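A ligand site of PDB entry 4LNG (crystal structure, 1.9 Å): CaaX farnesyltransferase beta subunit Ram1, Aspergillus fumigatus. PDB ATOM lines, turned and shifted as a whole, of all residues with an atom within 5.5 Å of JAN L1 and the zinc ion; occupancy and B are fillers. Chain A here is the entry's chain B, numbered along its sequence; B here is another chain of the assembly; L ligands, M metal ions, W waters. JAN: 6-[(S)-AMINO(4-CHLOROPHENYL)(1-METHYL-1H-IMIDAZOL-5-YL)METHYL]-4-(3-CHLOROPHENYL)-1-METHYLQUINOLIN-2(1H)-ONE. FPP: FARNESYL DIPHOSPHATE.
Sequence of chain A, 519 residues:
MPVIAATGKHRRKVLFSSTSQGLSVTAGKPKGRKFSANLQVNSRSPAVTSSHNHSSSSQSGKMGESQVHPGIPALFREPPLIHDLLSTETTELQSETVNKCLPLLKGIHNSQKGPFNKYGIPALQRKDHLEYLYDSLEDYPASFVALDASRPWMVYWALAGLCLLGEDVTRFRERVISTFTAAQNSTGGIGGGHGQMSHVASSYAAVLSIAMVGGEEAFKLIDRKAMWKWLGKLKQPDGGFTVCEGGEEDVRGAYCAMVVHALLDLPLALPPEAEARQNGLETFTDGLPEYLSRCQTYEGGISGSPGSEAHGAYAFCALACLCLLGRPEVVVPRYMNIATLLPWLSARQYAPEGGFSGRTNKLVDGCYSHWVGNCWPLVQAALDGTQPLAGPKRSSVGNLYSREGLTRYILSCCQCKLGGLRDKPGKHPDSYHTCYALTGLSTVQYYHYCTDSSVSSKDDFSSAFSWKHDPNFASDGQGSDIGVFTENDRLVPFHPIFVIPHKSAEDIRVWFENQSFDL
O3B of FPP L2 sits at hydrogen-bond distance from OH of Tyr 368, 2.7 Å away.
A ring nitrogen (ND1) of His 433 lies within hydrogen-bond range of the side-chain carboxylate (OD2) of Asp 430 (2.7 Å).
NE1 of Trp 371 lies within hydrogen-bond range of OH of Tyr 432, 3.1 Å away.
N of Tyr 432 sits at hydrogen-bond distance from OD1 of Asp 430, 3.0 Å away.
The side-chain sulfur of Cys 367 sits close to the side-chain hydroxyl of Tyr 432, 3.2 Å away.
Ser 150 touches JAN L1 (OG to C26, 3.4 Å).
Trp 153 touches JAN L1 (CD1 to C25, 3.7 Å).
Trp 157 touches JAN L1.
Tyr 368 touches JAN L1.
OD2 of Asp 430 touches C18 of JAN L1, at 3.5 Å.
Tyr 432 touches JAN L1.
Of the 16 residues printed, 9 come within 4 Å of JAN L1.
The nearest printed residue that does not touch JAN L1 is Leu 147 (4.1 Å).
Tyr 432 touches the zinc ion.
Within 4 Å of the zinc ion: Asp 365, Cys 367, Tyr 432 and His 433.
Along chain A the residues within 4 Å of the zinc ion span positions 365 to 433.
The nearest printed residue that does not touch the zinc ion is Asp 423 (4.4 Å).
The zinc ion is bound by a ring nitrogen (NE2) of His 433 (2.1 Å), the side-chain carboxylate (OD2) of Asp 365 (2.1 Å), a nitrogen (N2) of JAN L1 (2.2 Å), the side-chain sulfur (SG) of Cys 367 (2.3 Å) and the side-chain carboxylate (OD1) of Asp 365 (2.5 Å).
The zinc ion has five donor atoms within binding distance.
Water W1 lies within hydrogen-bond range of O1 of FPP L2 (2.9 Å) and N3 of JAN L1 (3.2 Å).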
ATOM      1  N   LEU A 147      34.058   8.979  -7.573  1.00  0.00           N
ATOM      2  CA  LEU A 147      34.707   8.811  -6.272  1.00  0.00           C
ATOM      3  C   LEU A 147      36.230   8.717  -6.377  1.00  0.00           C
ATOM      4  O   LEU A 147      36.911   8.533  -5.363  1.00  0.00           O
ATOM      5  CB  LEU A 147      34.161   7.571  -5.564  1.00  0.00           C
ATOM      6  CG  LEU A 147      32.695   7.648  -5.122  1.00  0.00           C
ATOM      7  CD1 LEU A 147      32.246   6.334  -4.485  1.00  0.00           C
ATOM      8  CD2 LEU A 147      32.496   8.806  -4.148  1.00  0.00           C
ATOM      9  N   SER A 150      38.250  10.666  -4.081  1.00  0.00           N
ATOM     10  CA  SER A 150      37.862  10.463  -2.683  1.00  0.00           C
ATOM     11  C   SER A 150      38.126   9.033  -2.201  1.00  0.00           C
ATOM     12  O   SER A 150      37.532   8.598  -1.208  1.00  0.00           O
ATOM     13  CB  SER A 150      36.390  10.817  -2.489  1.00  0.00           C
ATOM     14  OG  SER A 150      36.137  12.161  -2.853  1.00  0.00           O
ATOM     15  N   TRP A 153      38.944   8.524   1.482  1.00  0.00           N
ATOM     16  CA  TRP A 153      37.726   8.615   2.303  1.00  0.00           C
ATOM     17  C   TRP A 153      37.030   7.260   2.376  1.00  0.00           C
ATOM     18  O   TRP A 153      36.573   6.849   3.440  1.00  0.00           O
ATOM     19  CB  TRP A 153      36.742   9.631   1.711  1.00  0.00           C
ATOM     20  CG  TRP A 153      36.858  11.052   2.182  1.00  0.00           C
ATOM     21  CD1 TRP A 153      36.959  12.164   1.404  1.00  0.00           C
ATOM     22  CD2 TRP A 153      36.840  11.526   3.550  1.00  0.00           C
ATOM     23  NE1 TRP A 153      37.023  13.292   2.187  1.00  0.00           N
ATOM     24  CE2 TRP A 153      36.956  12.928   3.498  1.00  0.00           C
ATOM     25  CE3 TRP A 153      36.745  10.898   4.797  1.00  0.00           C
ATOM     26  CZ2 TRP A 153      36.980  13.719   4.652  1.00  0.00           C
ATOM     27  CZ3 TRP A 153      36.760  11.677   5.935  1.00  0.00           C
ATOM     28  CH2 TRP A 153      36.880  13.074   5.860  1.00  0.00           C
ATOM     29  N   TRP A 157      35.988   5.395   5.887  1.00  0.00           N
ATOM     30  CA  TRP A 157      34.593   5.149   6.263  1.00  0.00           C
ATOM     31  C   TRP A 157      34.360   3.671   6.568  1.00  0.00           C
ATOM     32  O   TRP A 157      33.688   3.322   7.549  1.00  0.00           O
ATOM     33  CB  TRP A 157      33.639   5.614   5.158  1.00  0.00           C
ATOM     34  CG  TRP A 157      33.650   7.099   4.912  1.00  0.00           C
ATOM     35  CD1 TRP A 157      33.826   8.084   5.845  1.00  0.00           C
ATOM     36  CD2 TRP A 157      33.489   7.757   3.656  1.00  0.00           C
ATOM     37  NE1 TRP A 157      33.785   9.324   5.229  1.00  0.00           N
ATOM     38  CE2 TRP A 157      33.578   9.146   3.886  1.00  0.00           C
ATOM     39  CE3 TRP A 157      33.279   7.311   2.341  1.00  0.00           C
ATOM     40  CZ2 TRP A 157      33.457  10.086   2.866  1.00  0.00           C
ATOM     41  CZ3 TRP A 157      33.165   8.247   1.331  1.00  0.00           C
ATOM     42  CH2 TRP A 157      33.251   9.624   1.598  1.00  0.00           C
ATOM     43  N   ARG A 252      36.246  23.136   7.145  1.00  0.00           N
ATOM     44  CA  ARG A 252      36.557  21.724   6.936  1.00  0.00           C
ATOM     45  C   ARG A 252      38.052  21.585   6.709  1.00  0.00           C
ATOM     46  O   ARG A 252      38.690  20.664   7.236  1.00  0.00           O
ATOM     47  CB  ARG A 252      35.774  21.172   5.740  1.00  0.00           C
ATOM     48  CG  ARG A 252      36.459  20.015   5.044  1.00  0.00           C
ATOM     49  CD  ARG A 252      35.828  19.727   3.688  1.00  0.00           C
ATOM     50  NE  ARG A 252      35.957  20.849   2.773  1.00  0.00           N
ATOM     51  CZ  ARG A 252      36.248  20.731   1.473  1.00  0.00           C
ATOM     52  NH1 ARG A 252      36.438  19.534   0.944  1.00  0.00           N
ATOM     53  NH2 ARG A 252      36.351  21.812   0.720  1.00  0.00           N
ATOM     54  N   ASP A 365      19.022  13.933   8.413  1.00  0.00           N
ATOM     55  CA  ASP A 365      19.964  13.135   7.642  1.00  0.00           C
ATOM     56  C   ASP A 365      20.819  12.354   8.635  1.00  0.00           C
ATOM     57  O   ASP A 365      21.409  12.928   9.543  1.00  0.00           O
ATOM     58  CB  ASP A 365      20.819  14.056   6.772  1.00  0.00           C
ATOM     59  CG  ASP A 365      21.869  13.319   5.940  1.00  0.00           C
ATOM     60  OD1 ASP A 365      22.230  12.163   6.262  1.00  0.00           O
ATOM     61  OD2 ASP A 365      22.355  13.920   4.959  1.00  0.00           O
ATOM     62  N   GLY A 366      20.886  11.034   8.448  1.00  0.00           N
ATOM     63  CA  GLY A 366      21.615  10.162   9.348  1.00  0.00           C
ATOM     64  C   GLY A 366      23.080  10.503   9.589  1.00  0.00           C
ATOM     65  O   GLY A 366      23.619  10.177  10.640  1.00  0.00           O
ATOM     66  N   CYS A 367      23.740  11.143   8.628  1.00  0.00           N
ATOM     67  CA  CYS A 367      25.150  11.471   8.823  1.00  0.00           C
ATOM     68  C   CYS A 367      25.340  12.574   9.860  1.00  0.00           C
ATOM     69  O   CYS A 367      26.398  12.677  10.479  1.00  0.00           O
ATOM     70  CB  CYS A 367      25.863  11.818   7.506  1.00  0.00           C
ATOM     71  SG  CYS A 367      25.432  13.412   6.757  1.00  0.00           S
ATOM     72  N   TYR A 368      24.315  13.396  10.058  1.00  0.00           N
ATOM     73  CA  TYR A 368      24.388  14.451  11.076  1.00  0.00           C
ATOM     74  C   TYR A 368      24.298  13.862  12.490  1.00  0.00           C
ATOM     75  O   TYR A 368      24.472  14.579  13.468  1.00  0.00           O
ATOM     76  CB  TYR A 368      23.328  15.531  10.821  1.00  0.00           C
ATOM     77  CG  TYR A 368      23.492  16.191   9.477  1.00  0.00           C
ATOM     78  CD1 TYR A 368      24.757  16.513   8.997  1.00  0.00           C
ATOM     79  CD2 TYR A 368      22.401  16.453   8.663  1.00  0.00           C
ATOM     80  CE1 TYR A 368      24.929  17.094   7.748  1.00  0.00           C
ATOM     81  CE2 TYR A 368      22.558  17.042   7.410  1.00  0.00           C
ATOM     82  CZ  TYR A 368      23.828  17.358   6.969  1.00  0.00           C
ATOM     83  OH  TYR A 368      24.008  17.935   5.732  1.00  0.00           O
ATOM     84  N   TRP A 371      27.930  14.651  12.728  1.00  0.00           N
ATOM     85  CA  TRP A 371      28.295  16.077  12.608  1.00  0.00           C
ATOM     86  C   TRP A 371      27.628  16.938  13.672  1.00  0.00           C
ATOM     87  O   TRP A 371      28.281  17.753  14.316  1.00  0.00           O
ATOM     88  CB  TRP A 371      28.029  16.625  11.199  1.00  0.00           C
ATOM     89  CG  TRP A 371      28.731  15.841  10.117  1.00  0.00           C
ATOM     90  CD1 TRP A 371      28.137  15.089   9.139  1.00  0.00           C
ATOM     91  CD2 TRP A 371      30.145  15.705   9.933  1.00  0.00           C
ATOM     92  NE1 TRP A 371      29.104  14.506   8.352  1.00  0.00           N
ATOM     93  CE2 TRP A 371      30.345  14.857   8.820  1.00  0.00           C
ATOM     94  CE3 TRP A 371      31.262  16.201  10.601  1.00  0.00           C
ATOM     95  CZ2 TRP A 371      31.609  14.509   8.352  1.00  0.00           C
ATOM     96  CZ3 TRP A 371      32.527  15.862  10.144  1.00  0.00           C
ATOM     97  CH2 TRP A 371      32.684  15.023   9.030  1.00  0.00           C
ATOM     98  N   ASP A 423      21.153   7.977   4.462  1.00  0.00           N
ATOM     99  CA  ASP A 423      20.773   9.350   4.773  1.00  0.00           C
ATOM    100  C   ASP A 423      19.377   9.356   5.413  1.00  0.00           C
ATOM    101  O   ASP A 423      19.196   9.827   6.526  1.00  0.00           O
ATOM    102  CB  ASP A 423      20.808  10.148   3.456  1.00  0.00           C
ATOM    103  CG  ASP A 423      20.198  11.546   3.536  1.00  0.00           C
ATOM    104  OD1 ASP A 423      19.510  11.905   4.522  1.00  0.00           O
ATOM    105  OD2 ASP A 423      20.390  12.301   2.564  1.00  0.00           O
ATOM    106  N   ASP A 430      25.161   4.106   1.592  1.00  0.00           N
ATOM    107  CA  ASP A 430      26.529   4.266   1.106  1.00  0.00           C
ATOM    108  C   ASP A 430      27.461   4.182   2.315  1.00  0.00           C
ATOM    109  O   ASP A 430      26.995   4.240   3.450  1.00  0.00           O
ATOM    110  CB  ASP A 430      26.708   5.581   0.341  1.00  0.00           C
ATOM    111  CG  ASP A 430      26.367   6.802   1.177  1.00  0.00           C
ATOM    112  OD1 ASP A 430      27.214   7.204   2.006  1.00  0.00           O
ATOM    113  OD2 ASP A 430      25.266   7.358   0.997  1.00  0.00           O
ATOM    114  N   SER A 431      28.754   4.023   2.075  1.00  0.00           N
ATOM    115  CA  SER A 431      29.672   3.796   3.181  1.00  0.00           C
ATOM    116  C   SER A 431      29.881   5.059   4.030  1.00  0.00           C
ATOM    117  O   SER A 431      30.191   4.967   5.209  1.00  0.00           O
ATOM    118  CB  SER A 431      31.001   3.202   2.714  1.00  0.00           C
ATOM    119  OG  SER A 431      31.717   4.094   1.884  1.00  0.00           O
ATOM    120  N   TYR A 432      29.710   6.228   3.414  1.00  0.00           N
ATOM    121  CA  TYR A 432      29.785   7.500   4.138  1.00  0.00           C
ATOM    122  C   TYR A 432      28.676   7.589   5.180  1.00  0.00           C
ATOM    123  O   TYR A 432      28.932   7.862   6.362  1.00  0.00           O
ATOM    124  CB  TYR A 432      29.731   8.685   3.154  1.00  0.00           C
ATOM    125  CG  TYR A 432      29.372  10.022   3.795  1.00  0.00           C
ATOM    126  CD1 TYR A 432      30.356  10.877   4.268  1.00  0.00           C
ATOM    127  CD2 TYR A 432      28.048  10.434   3.890  1.00  0.00           C
ATOM    128  CE1 TYR A 432      30.030  12.103   4.846  1.00  0.00           C
ATOM    129  CE2 TYR A 432      27.707  11.644   4.464  1.00  0.00           C
ATOM    130  CZ  TYR A 432      28.698  12.479   4.942  1.00  0.00           C
ATOM    131  OH  TYR A 432      28.349  13.693   5.506  1.00  0.00           O
ATOM    132  N   HIS A 433      27.437   7.350   4.760  1.00  0.00           N
ATOM    133  CA  HIS A 433      26.306   7.406   5.677  1.00  0.00           C
ATOM    134  C   HIS A 433      26.313   6.251   6.671  1.00  0.00           C
ATOM    135  O   HIS A 433      25.840   6.386   7.793  1.00  0.00           O
ATOM    136  CB  HIS A 433      24.974   7.495   4.918  1.00  0.00           C
ATOM    137  CG  HIS A 433      24.705   8.852   4.340  1.00  0.00           C
ATOM    138  ND1 HIS A 433      24.852   9.132   2.995  1.00  0.00           N
ATOM    139  CD2 HIS A 433      24.343  10.010   4.930  1.00  0.00           C
ATOM    140  CE1 HIS A 433      24.570  10.401   2.782  1.00  0.00           C
ATOM    141  NE2 HIS A 433      24.261  10.963   3.940  1.00  0.00           N
ATOM    142  N   TYR B 123      30.483  21.298  -6.329  1.00  0.00           N
ATOM    143  CA  TYR B 123      30.978  22.537  -5.730  1.00  0.00           C
ATOM    144  C   TYR B 123      32.342  22.994  -6.255  1.00  0.00           C
ATOM    145  O   TYR B 123      32.693  24.164  -6.115  1.00  0.00           O
ATOM    146  CB  TYR B 123      30.971  22.457  -4.198  1.00  0.00           C
ATOM    147  CG  TYR B 123      31.940  21.449  -3.610  1.00  0.00           C
ATOM    148  CD1 TYR B 123      33.252  21.803  -3.342  1.00  0.00           C
ATOM    149  CD2 TYR B 123      31.526  20.154  -3.315  1.00  0.00           C
ATOM    150  CE1 TYR B 123      34.134  20.886  -2.794  1.00  0.00           C
ATOM    151  CE2 TYR B 123      32.414  19.232  -2.774  1.00  0.00           C
ATOM    152  CZ  TYR B 123      33.711  19.602  -2.516  1.00  0.00           C
ATOM    153  OH  TYR B 123      34.606  18.701  -1.982  1.00  0.00           O
HETATM  154  C1  JAN L   1      25.751  17.453   2.160  1.00  0.00           C
HETATM  155  N1  JAN L   1      25.815  15.945   2.387  1.00  0.00           N
HETATM  156  C2  JAN L   1      25.091  15.479   3.367  1.00  0.00           C
HETATM  157  N2  JAN L   1      25.089  14.223   3.319  1.00  0.00           N
HETATM  158  C3  JAN L   1      25.914  13.624   2.339  1.00  0.00           C
HETATM  159  C4  JAN L   1      26.239  14.849   1.562  1.00  0.00           C
HETATM  160  C5  JAN L   1      27.260  14.977   0.249  1.00  0.00           C
HETATM  161  C6  JAN L   1      28.407  15.912   0.764  1.00  0.00           C
HETATM  162  C7  JAN L   1      29.002  15.597   1.943  1.00  0.00           C
HETATM  163  C8  JAN L   1      30.201  16.150   2.431  1.00  0.00           C
HETATM  164  C9  JAN L   1      30.621  16.964   1.188  1.00  0.00           C
HETATM  165 CL1  JAN L   1      32.367  17.629   1.718  1.00  0.00          CL
HETATM  166  C10 JAN L   1      30.137  17.280   0.119  1.00  0.00           C
HETATM  167  C11 JAN L   1      28.845  16.688  -0.166  1.00  0.00           C
HETATM  168  N3  JAN L   1      26.484  15.815  -0.610  1.00  0.00           N
HETATM  169  C12 JAN L   1      27.517  13.497  -0.045  1.00  0.00           C
HETATM  170  C13 JAN L   1      28.723  13.148  -0.065  1.00  0.00           C
HETATM  171  C14 JAN L   1      28.937  11.900  -0.613  1.00  0.00           C
HETATM  172  C15 JAN L   1      26.377  12.945  -0.587  1.00  0.00           C
HETATM  173  C16 JAN L   1      26.567  11.408  -1.034  1.00  0.00           C
HETATM  174  C17 JAN L   1      28.069  11.069  -0.814  1.00  0.00           C
HETATM  175  N4  JAN L   1      28.180   9.717  -1.375  1.00  0.00           N
HETATM  176  C18 JAN L   1      26.915   8.860  -1.747  1.00  0.00           C
HETATM  177  C19 JAN L   1      29.380   9.110  -1.188  1.00  0.00           C
HETATM  178  O1  JAN L   1      29.452   7.909  -1.547  1.00  0.00           O
HETATM  179  C20 JAN L   1      30.364   9.999  -0.787  1.00  0.00           C
HETATM  180  C21 JAN L   1      30.296  11.335  -0.613  1.00  0.00           C
HETATM  181  C22 JAN L   1      31.433  12.138  -0.155  1.00  0.00           C
HETATM  182  C23 JAN L   1      31.503  12.578   1.245  1.00  0.00           C
HETATM  183  C24 JAN L   1      32.678  13.287   1.411  1.00  0.00           C
HETATM  184 CL2  JAN L   1      32.879  13.914   3.063  1.00  0.00          CL
HETATM  185  C25 JAN L   1      33.724  13.766   0.443  1.00  0.00           C
HETATM  186  C26 JAN L   1      33.564  13.047  -0.804  1.00  0.00           C
HETATM  187  C27 JAN L   1      32.449  12.405  -1.019  1.00  0.00           C
HETATM  188  C1  FPP L   2      25.151  21.101   1.988  1.00  0.00           C
HETATM  189  O1  FPP L   2      24.656  20.192   1.046  1.00  0.00           O
HETATM  190  C2  FPP L   2      26.052  20.652   2.935  1.00  0.00           C
HETATM  191  C3  FPP L   2      27.205  21.495   3.395  1.00  0.00           C
HETATM  192  C4  FPP L   2      27.884  22.134   2.217  1.00  0.00           C
HETATM  193  C5  FPP L   2      28.160  20.634   4.275  1.00  0.00           C
HETATM  194  C6  FPP L   2      28.975  19.515   3.588  1.00  0.00           C
HETATM  195  C7  FPP L   2      30.089  18.923   4.232  1.00  0.00           C
HETATM  196  C8  FPP L   2      29.899  18.026   5.447  1.00  0.00           C
HETATM  197  C10 FPP L   2      28.811  17.012   5.236  1.00  0.00           C
HETATM  198  C9  FPP L   2      31.192  17.399   5.916  1.00  0.00           C
HETATM  199  C11 FPP L   2      32.385  18.311   6.067  1.00  0.00           C
HETATM  200  C12 FPP L   2      33.440  17.957   6.895  1.00  0.00           C
HETATM  201  C13 FPP L   2      34.390  16.823   6.542  1.00  0.00           C
HETATM  202  C14 FPP L   2      34.688  16.665   5.056  1.00  0.00           C
HETATM  203  C15 FPP L   2      35.585  16.689   7.434  1.00  0.00           C
HETATM  204  PA  FPP L   2      23.136  19.735   1.054  1.00  0.00           P
HETATM  205  O1A FPP L   2      22.264  20.904   0.671  1.00  0.00           O
HETATM  206  O2A FPP L   2      22.978  18.633   0.048  1.00  0.00           O
HETATM  207  O3A FPP L   2      22.805  19.159   2.471  1.00  0.00           O
HETATM  208  PB  FPP L   2      21.780  19.777   3.507  1.00  0.00           P
HETATM  209  O1B FPP L   2      20.396  19.923   2.909  1.00  0.00           O
HETATM  210  O2B FPP L   2      22.254  21.111   4.018  1.00  0.00           O
HETATM  211  O3B FPP L   2      21.694  18.786   4.657  1.00  0.00           O
HETATM  212 ZN    ZN M   1      24.200  12.882   4.830  1.00  0.00          ZN
HETATM  213  O   HOH W   1      26.101  18.919  -1.081  1.00  0.00           O
HETATM  214  O   HOH W   2      27.181  15.603  -3.270  1.00  0.00           O
HETATM  215  O   HOH W   3      23.259  14.213  -1.037  1.00  0.00           O
